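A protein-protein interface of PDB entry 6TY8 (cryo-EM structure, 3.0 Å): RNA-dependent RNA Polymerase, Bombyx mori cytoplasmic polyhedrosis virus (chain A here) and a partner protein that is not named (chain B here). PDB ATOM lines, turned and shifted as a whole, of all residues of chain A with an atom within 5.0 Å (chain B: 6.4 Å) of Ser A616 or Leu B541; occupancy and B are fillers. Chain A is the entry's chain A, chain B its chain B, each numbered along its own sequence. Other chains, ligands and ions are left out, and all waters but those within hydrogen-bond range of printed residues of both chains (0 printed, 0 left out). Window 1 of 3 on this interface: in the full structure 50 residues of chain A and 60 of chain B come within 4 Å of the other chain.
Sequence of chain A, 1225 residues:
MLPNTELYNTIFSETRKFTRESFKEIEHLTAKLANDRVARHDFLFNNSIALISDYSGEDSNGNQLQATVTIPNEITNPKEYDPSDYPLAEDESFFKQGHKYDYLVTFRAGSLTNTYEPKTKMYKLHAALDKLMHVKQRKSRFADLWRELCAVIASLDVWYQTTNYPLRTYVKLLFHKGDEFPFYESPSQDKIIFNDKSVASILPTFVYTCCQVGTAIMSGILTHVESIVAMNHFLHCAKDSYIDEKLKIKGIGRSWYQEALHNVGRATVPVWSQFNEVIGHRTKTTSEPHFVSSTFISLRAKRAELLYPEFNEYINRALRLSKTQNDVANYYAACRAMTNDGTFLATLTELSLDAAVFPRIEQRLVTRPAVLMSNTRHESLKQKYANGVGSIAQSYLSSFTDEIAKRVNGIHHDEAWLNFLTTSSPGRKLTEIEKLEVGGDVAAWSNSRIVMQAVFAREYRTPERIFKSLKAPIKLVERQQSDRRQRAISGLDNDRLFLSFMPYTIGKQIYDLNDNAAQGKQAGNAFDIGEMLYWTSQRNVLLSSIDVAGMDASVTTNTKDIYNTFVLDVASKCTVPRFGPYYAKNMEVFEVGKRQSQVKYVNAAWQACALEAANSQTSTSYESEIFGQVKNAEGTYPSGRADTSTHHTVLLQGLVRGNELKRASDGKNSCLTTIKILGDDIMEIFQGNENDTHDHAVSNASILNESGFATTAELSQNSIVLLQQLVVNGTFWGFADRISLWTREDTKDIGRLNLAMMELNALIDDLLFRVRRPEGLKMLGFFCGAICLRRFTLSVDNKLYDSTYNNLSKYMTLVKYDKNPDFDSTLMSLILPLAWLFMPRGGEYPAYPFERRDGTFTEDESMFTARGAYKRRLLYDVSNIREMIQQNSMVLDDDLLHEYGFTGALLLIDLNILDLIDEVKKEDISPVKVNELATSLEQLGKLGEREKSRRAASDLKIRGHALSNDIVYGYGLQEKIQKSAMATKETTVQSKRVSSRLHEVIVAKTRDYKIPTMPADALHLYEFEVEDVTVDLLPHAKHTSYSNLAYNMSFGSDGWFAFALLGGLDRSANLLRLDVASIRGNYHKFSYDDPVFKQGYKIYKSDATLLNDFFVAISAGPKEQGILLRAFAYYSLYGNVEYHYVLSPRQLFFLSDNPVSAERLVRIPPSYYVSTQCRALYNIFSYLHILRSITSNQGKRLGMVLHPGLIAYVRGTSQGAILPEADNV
O of Ala A614 sits close to N of His B542 (3.4 Å).
O of Ser A616 sits at hydrogen-bond distance from ND1 of His B542 (3.0 Å).
The backbone carbonyl oxygen of Leu B541 sits close to the backbone carbonyl oxygen of Ala A614 (3.0 Å).
N of Ser A616 sits at hydrogen-bond distance from O of Leu B541, at 3.4 Å.
The side-chain carboxylate of Glu A634 sits at hydrogen-bond distance from the backbone NH of Thr A618, 2.4 Å away.
N of Leu B506 is in hydrogen-bond range of O of Thr B543, 2.8 Å away.
The side-chain amide oxygen (OD1) of Asn B492 lies close to the backbone carbonyl oxygen (O) of Pro B539.
O of Thr A557 touches CD1 of Leu B541, at 3.3 Å.
Asn B492 touches Asn A558.
Pro B539 touches Asn A558 (CD to OD1, 3.2 Å).
OD2 of Asp A561 touches CG of Pro B539 (3.9 Å).
OD2 of Asp A561 touches CD1 of Leu B541, at 3.9 Å.
Ala A613 touches Leu B541.
Thr B543 touches Ala A614.
OD1 of Asn A615 touches CG2 of Thr B543 (3.5 Å).
Thr B504 touches Gln A617 (CG2 to NE2, 3.4 Å).
Glu A634 touches Thr B504.
Printed residues of chain B within 4 Å of Thr A557: Leu B541.
Printed residues of chain B within 4 Å of Asp A561: Pro B539 (3.9 Å) and Leu B541 (3.9 Å).
Of the printed residues of chain B, Ala A614 touches Leu B541 (3.0 Å), His B542 (3.1 Å) and Thr B543 (3.8 Å).
Ser A616 touches two residues of chain B.
Of the printed residues of chain A, Asn B492 touches Asn A558.
Of the printed residues of chain A, Pro B539 touches Asn A558 (3.2 Å) and Asp A561 (3.9 Å).
Of chain A, only Thr A557, Asp A561, Ala A613, Ala A614 and Ser A616 come within 4 Å of Leu B541.
The nearest residue of chain B that does not touch Ser A616 is Thr B504 (5.0 Å).
The nearest printed residue of chain A that does not touch Pro B539 is Thr A557 (6.1 Å).
Of the 9 printed residues of chain B, 6 touch a printed residue of chain A.
Hydrophobic or aromatic side chains of chain B within 4 Å of the printed part of chain A: Pro B539, Leu B541 and His B542.
Among the printed residues, 15 pairs touch across the chains.
Among the printed residues, no Asp or Glu carboxylate lies within 4 Å of a Lys or Arg side-chain nitrogen of the other chain.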
ATOM      1  N   THR A 557       3.666  -6.768  25.705  1.00  0.00           N
ATOM      2  CA  THR A 557       4.472  -7.974  25.840  1.00  0.00           C
ATOM      3  C   THR A 557       3.696  -9.065  26.568  1.00  0.00           C
ATOM      4  O   THR A 557       3.794 -10.244  26.214  1.00  0.00           O
ATOM      5  CB  THR A 557       5.773  -7.641  26.571  1.00  0.00           C
ATOM      6  OG1 THR A 557       6.422  -6.553  25.905  1.00  0.00           O
ATOM      7  CG2 THR A 557       6.714  -8.825  26.556  1.00  0.00           C
ATOM      8  N   ASN A 558       2.880  -8.686  27.551  1.00  0.00           N
ATOM      9  CA  ASN A 558       2.025  -9.659  28.212  1.00  0.00           C
ATOM     10  C   ASN A 558       0.803 -10.017  27.386  1.00  0.00           C
ATOM     11  O   ASN A 558       0.180 -11.053  27.639  1.00  0.00           O
ATOM     12  CB  ASN A 558       1.574  -9.135  29.564  1.00  0.00           C
ATOM     13  CG  ASN A 558       2.724  -8.871  30.486  1.00  0.00           C
ATOM     14  OD1 ASN A 558       3.758  -9.512  30.382  1.00  0.00           O
ATOM     15  ND2 ASN A 558       2.537  -7.959  31.429  1.00  0.00           N
ATOM     16  N   ASP A 561       1.697 -12.957  25.245  1.00  0.00           N
ATOM     17  CA  ASP A 561       1.845 -14.198  25.985  1.00  0.00           C
ATOM     18  C   ASP A 561       0.594 -15.067  25.927  1.00  0.00           C
ATOM     19  O   ASP A 561       0.675 -16.253  26.250  1.00  0.00           O
ATOM     20  CB  ASP A 561       2.209 -13.873  27.430  1.00  0.00           C
ATOM     21  CG  ASP A 561       2.958 -14.994  28.112  1.00  0.00           C
ATOM     22  OD1 ASP A 561       3.203 -16.040  27.480  1.00  0.00           O
ATOM     23  OD2 ASP A 561       3.341 -14.814  29.283  1.00  0.00           O
ATOM     24  N   ASN A 564       1.553 -16.996  22.936  1.00  0.00           N
ATOM     25  CA  ASN A 564       2.700 -17.842  23.249  1.00  0.00           C
ATOM     26  C   ASN A 564       2.278 -19.164  23.885  1.00  0.00           C
ATOM     27  O   ASN A 564       2.887 -20.202  23.607  1.00  0.00           O
ATOM     28  CB  ASN A 564       3.675 -17.099  24.158  1.00  0.00           C
ATOM     29  CG  ASN A 564       4.432 -16.022  23.428  1.00  0.00           C
ATOM     30  OD1 ASN A 564       4.833 -16.203  22.281  1.00  0.00           O
ATOM     31  ND2 ASN A 564       4.644 -14.897  24.090  1.00  0.00           N
ATOM     32  N   GLU A 612      12.224 -18.011  20.750  1.00  0.00           N
ATOM     33  CA  GLU A 612      11.631 -16.799  20.201  1.00  0.00           C
ATOM     34  C   GLU A 612      10.638 -16.169  21.164  1.00  0.00           C
ATOM     35  O   GLU A 612      10.474 -14.945  21.161  1.00  0.00           O
ATOM     36  CB  GLU A 612      10.962 -17.113  18.863  1.00  0.00           C
ATOM     37  CG  GLU A 612      10.554 -15.912  18.027  1.00  0.00           C
ATOM     38  CD  GLU A 612       9.146 -15.437  18.308  1.00  0.00           C
ATOM     39  OE1 GLU A 612       8.310 -16.269  18.720  1.00  0.00           O
ATOM     40  OE2 GLU A 612       8.873 -14.238  18.105  1.00  0.00           O
ATOM     41  N   ALA A 613       9.977 -16.971  21.997  1.00  0.00           N
ATOM     42  CA  ALA A 613       9.081 -16.399  22.993  1.00  0.00           C
ATOM     43  C   ALA A 613       9.855 -15.758  24.130  1.00  0.00           C
ATOM     44  O   ALA A 613       9.428 -14.732  24.666  1.00  0.00           O
ATOM     45  CB  ALA A 613       8.134 -17.463  23.542  1.00  0.00           C
ATOM     46  N   ALA A 614      10.987 -16.341  24.517  1.00  0.00           N
ATOM     47  CA  ALA A 614      11.728 -15.787  25.642  1.00  0.00           C
ATOM     48  C   ALA A 614      12.580 -14.598  25.234  1.00  0.00           C
ATOM     49  O   ALA A 614      12.887 -13.746  26.072  1.00  0.00           O
ATOM     50  CB  ALA A 614      12.600 -16.862  26.276  1.00  0.00           C
ATOM     51  N   ASN A 615      13.012 -14.528  23.982  1.00  0.00           N
ATOM     52  CA  ASN A 615      13.795 -13.370  23.569  1.00  0.00           C
ATOM     53  C   ASN A 615      12.918 -12.503  22.686  1.00  0.00           C
ATOM     54  O   ASN A 615      12.699 -12.823  21.520  1.00  0.00           O
ATOM     55  CB  ASN A 615      15.033 -13.817  22.803  1.00  0.00           C
ATOM     56  CG  ASN A 615      15.851 -14.832  23.567  1.00  0.00           C
ATOM     57  OD1 ASN A 615      16.058 -14.699  24.769  1.00  0.00           O
ATOM     58  ND2 ASN A 615      16.322 -15.856  22.870  1.00  0.00           N
ATOM     59  N   SER A 616      12.431 -11.393  23.227  1.00  0.00           N
ATOM     60  CA  SER A 616      11.562 -10.524  22.446  1.00  0.00           C
ATOM     61  C   SER A 616      11.907  -9.040  22.453  1.00  0.00           C
ATOM     62  O   SER A 616      12.000  -8.420  23.510  1.00  0.00           O
ATOM     63  CB  SER A 616      10.116 -10.701  22.907  1.00  0.00           C
ATOM     64  OG  SER A 616       9.282  -9.715  22.333  1.00  0.00           O
ATOM     65  N   GLN A 617      12.104  -8.491  21.262  1.00  0.00           N
ATOM     66  CA  GLN A 617      12.328  -7.071  21.124  1.00  0.00           C
ATOM     67  C   GLN A 617      11.361  -6.585  20.056  1.00  0.00           C
ATOM     68  O   GLN A 617      11.409  -7.052  18.920  1.00  0.00           O
ATOM     69  CB  GLN A 617      13.767  -6.782  20.711  1.00  0.00           C
ATOM     70  CG  GLN A 617      14.244  -5.398  21.112  1.00  0.00           C
ATOM     71  CD  GLN A 617      14.333  -5.237  22.617  1.00  0.00           C
ATOM     72  OE1 GLN A 617      14.944  -6.055  23.302  1.00  0.00           O
ATOM     73  NE2 GLN A 617      13.724  -4.181  23.138  1.00  0.00           N
ATOM     74  N   THR A 618      10.488  -5.648  20.405  1.00  0.00           N
ATOM     75  CA  THR A 618       9.550  -5.101  19.426  1.00  0.00           C
ATOM     76  C   THR A 618       9.851  -3.675  18.942  1.00  0.00           C
ATOM     77  O   THR A 618       9.128  -3.149  18.099  1.00  0.00           O
ATOM     78  CB  THR A 618       8.094  -5.167  19.928  1.00  0.00           C
ATOM     79  OG1 THR A 618       7.927  -4.292  21.050  1.00  0.00           O
ATOM     80  CG2 THR A 618       7.737  -6.587  20.332  1.00  0.00           C
ATOM     81  N   GLU A 634       9.987   0.042  23.739  1.00  0.00           N
ATOM     82  CA  GLU A 634       9.701  -1.368  23.545  1.00  0.00           C
ATOM     83  C   GLU A 634       8.238  -1.643  23.866  1.00  0.00           C
ATOM     84  O   GLU A 634       7.714  -1.158  24.866  1.00  0.00           O
ATOM     85  CB  GLU A 634      10.605  -2.219  24.438  1.00  0.00           C
ATOM     86  CG  GLU A 634      11.140  -3.479  23.776  1.00  0.00           C
ATOM     87  CD  GLU A 634      10.055  -4.486  23.452  1.00  0.00           C
ATOM     88  OE1 GLU A 634       8.896  -4.265  23.850  1.00  0.00           O
ATOM     89  OE2 GLU A 634      10.366  -5.502  22.800  1.00  0.00           O
ATOM     90  N   ASN B 492       6.858  -5.892  33.083  1.00  0.00           N
ATOM     91  CA  ASN B 492       6.914  -5.732  31.633  1.00  0.00           C
ATOM     92  C   ASN B 492       5.964  -4.670  31.103  1.00  0.00           C
ATOM     93  O   ASN B 492       6.097  -4.270  29.945  1.00  0.00           O
ATOM     94  CB  ASN B 492       6.602  -7.043  30.911  1.00  0.00           C
ATOM     95  CG  ASN B 492       7.678  -8.077  31.076  1.00  0.00           C
ATOM     96  OD1 ASN B 492       7.442  -9.158  31.590  1.00  0.00           O
ATOM     97  ND2 ASN B 492       8.878  -7.747  30.644  1.00  0.00           N
ATOM     98  N   THR B 504      16.531  -4.365  26.094  1.00  0.00           N
ATOM     99  CA  THR B 504      15.993  -4.558  27.431  1.00  0.00           C
ATOM    100  C   THR B 504      16.203  -6.010  27.835  1.00  0.00           C
ATOM    101  O   THR B 504      16.037  -6.922  27.022  1.00  0.00           O
ATOM    102  CB  THR B 504      14.511  -4.138  27.522  1.00  0.00           C
ATOM    103  OG1 THR B 504      13.999  -4.429  28.829  1.00  0.00           O
ATOM    104  CG2 THR B 504      13.661  -4.794  26.465  1.00  0.00           C
ATOM    105  N   LEU B 506      16.314  -9.128  31.216  1.00  0.00           N
ATOM    106  CA  LEU B 506      15.791  -9.590  32.495  1.00  0.00           C
ATOM    107  C   LEU B 506      16.939 -10.222  33.264  1.00  0.00           C
ATOM    108  O   LEU B 506      17.794 -10.887  32.675  1.00  0.00           O
ATOM    109  CB  LEU B 506      14.638 -10.580  32.310  1.00  0.00           C
ATOM    110  CG  LEU B 506      13.726 -10.882  33.507  1.00  0.00           C
ATOM    111  CD1 LEU B 506      12.340 -11.154  32.996  1.00  0.00           C
ATOM    112  CD2 LEU B 506      14.185 -12.062  34.327  1.00  0.00           C
ATOM    113  N   LEU B 538       5.313  -9.719  35.801  1.00  0.00           N
ATOM    114  CA  LEU B 538       6.588  -9.857  35.089  1.00  0.00           C
ATOM    115  C   LEU B 538       6.814 -11.298  34.636  1.00  0.00           C
ATOM    116  O   LEU B 538       7.371 -12.118  35.379  1.00  0.00           O
ATOM    117  CB  LEU B 538       7.754  -9.380  35.959  1.00  0.00           C
ATOM    118  CG  LEU B 538       9.177  -9.382  35.393  1.00  0.00           C
ATOM    119  CD1 LEU B 538       9.334  -8.421  34.253  1.00  0.00           C
ATOM    120  CD2 LEU B 538      10.172  -9.063  36.478  1.00  0.00           C
ATOM    121  N   PRO B 539       6.376 -11.645  33.430  1.00  0.00           N
ATOM    122  CA  PRO B 539       6.851 -12.875  32.794  1.00  0.00           C
ATOM    123  C   PRO B 539       8.314 -12.773  32.401  1.00  0.00           C
ATOM    124  O   PRO B 539       8.914 -11.699  32.365  1.00  0.00           O
ATOM    125  CB  PRO B 539       5.969 -12.993  31.553  1.00  0.00           C
ATOM    126  CG  PRO B 539       4.773 -12.253  31.877  1.00  0.00           C
ATOM    127  CD  PRO B 539       5.173 -11.133  32.764  1.00  0.00           C
ATOM    128  N   ALA B 540       8.887 -13.926  32.079  1.00  0.00           N
ATOM    129  CA  ALA B 540      10.266 -13.994  31.602  1.00  0.00           C
ATOM    130  C   ALA B 540      10.232 -13.956  30.083  1.00  0.00           C
ATOM    131  O   ALA B 540      10.518 -14.944  29.408  1.00  0.00           O
ATOM    132  CB  ALA B 540      10.960 -15.245  32.120  1.00  0.00           C
ATOM    133  N   LEU B 541       9.883 -12.794  29.537  1.00  0.00           N
ATOM    134  CA  LEU B 541       9.727 -12.632  28.104  1.00  0.00           C
ATOM    135  C   LEU B 541      10.824 -11.801  27.460  1.00  0.00           C
ATOM    136  O   LEU B 541      10.798 -11.616  26.244  1.00  0.00           O
ATOM    137  CB  LEU B 541       8.360 -12.023  27.787  1.00  0.00           C
ATOM    138  CG  LEU B 541       7.191 -12.975  28.035  1.00  0.00           C
ATOM    139  CD1 LEU B 541       5.866 -12.281  27.841  1.00  0.00           C
ATOM    140  CD2 LEU B 541       7.287 -14.179  27.131  1.00  0.00           C
ATOM    141  N   HIS B 542      11.789 -11.303  28.226  1.00  0.00           N
ATOM    142  CA  HIS B 542      12.982 -10.696  27.658  1.00  0.00           C
ATOM    143  C   HIS B 542      14.185 -11.569  27.991  1.00  0.00           C
ATOM    144  O   HIS B 542      14.057 -12.587  28.672  1.00  0.00           O
ATOM    145  CB  HIS B 542      13.179  -9.268  28.161  1.00  0.00           C
ATOM    146  CG  HIS B 542      12.103  -8.326  27.726  1.00  0.00           C
ATOM    147  ND1 HIS B 542      11.975  -7.894  26.424  1.00  0.00           N
ATOM    148  CD2 HIS B 542      11.114  -7.720  28.420  1.00  0.00           C
ATOM    149  CE1 HIS B 542      10.945  -7.074  26.333  1.00  0.00           C
ATOM    150  NE2 HIS B 542      10.407  -6.949  27.531  1.00  0.00           N
ATOM    151  N   THR B 543      15.357 -11.175  27.493  1.00  0.00           N
ATOM    152  CA  THR B 543      16.510 -12.067  27.536  1.00  0.00           C
ATOM    153  C   THR B 543      17.067 -12.177  28.948  1.00  0.00           C
ATOM    154  O   THR B 543      17.415 -11.178  29.577  1.00  0.00           O
ATOM    155  CB  THR B 543      17.606 -11.581  26.596  1.00  0.00           C
ATOM    156  OG1 THR B 543      18.118 -10.338  27.075  1.00  0.00           O
ATOM    157  CG2 THR B 543      17.060 -11.377  25.209  1.00  0.00           C
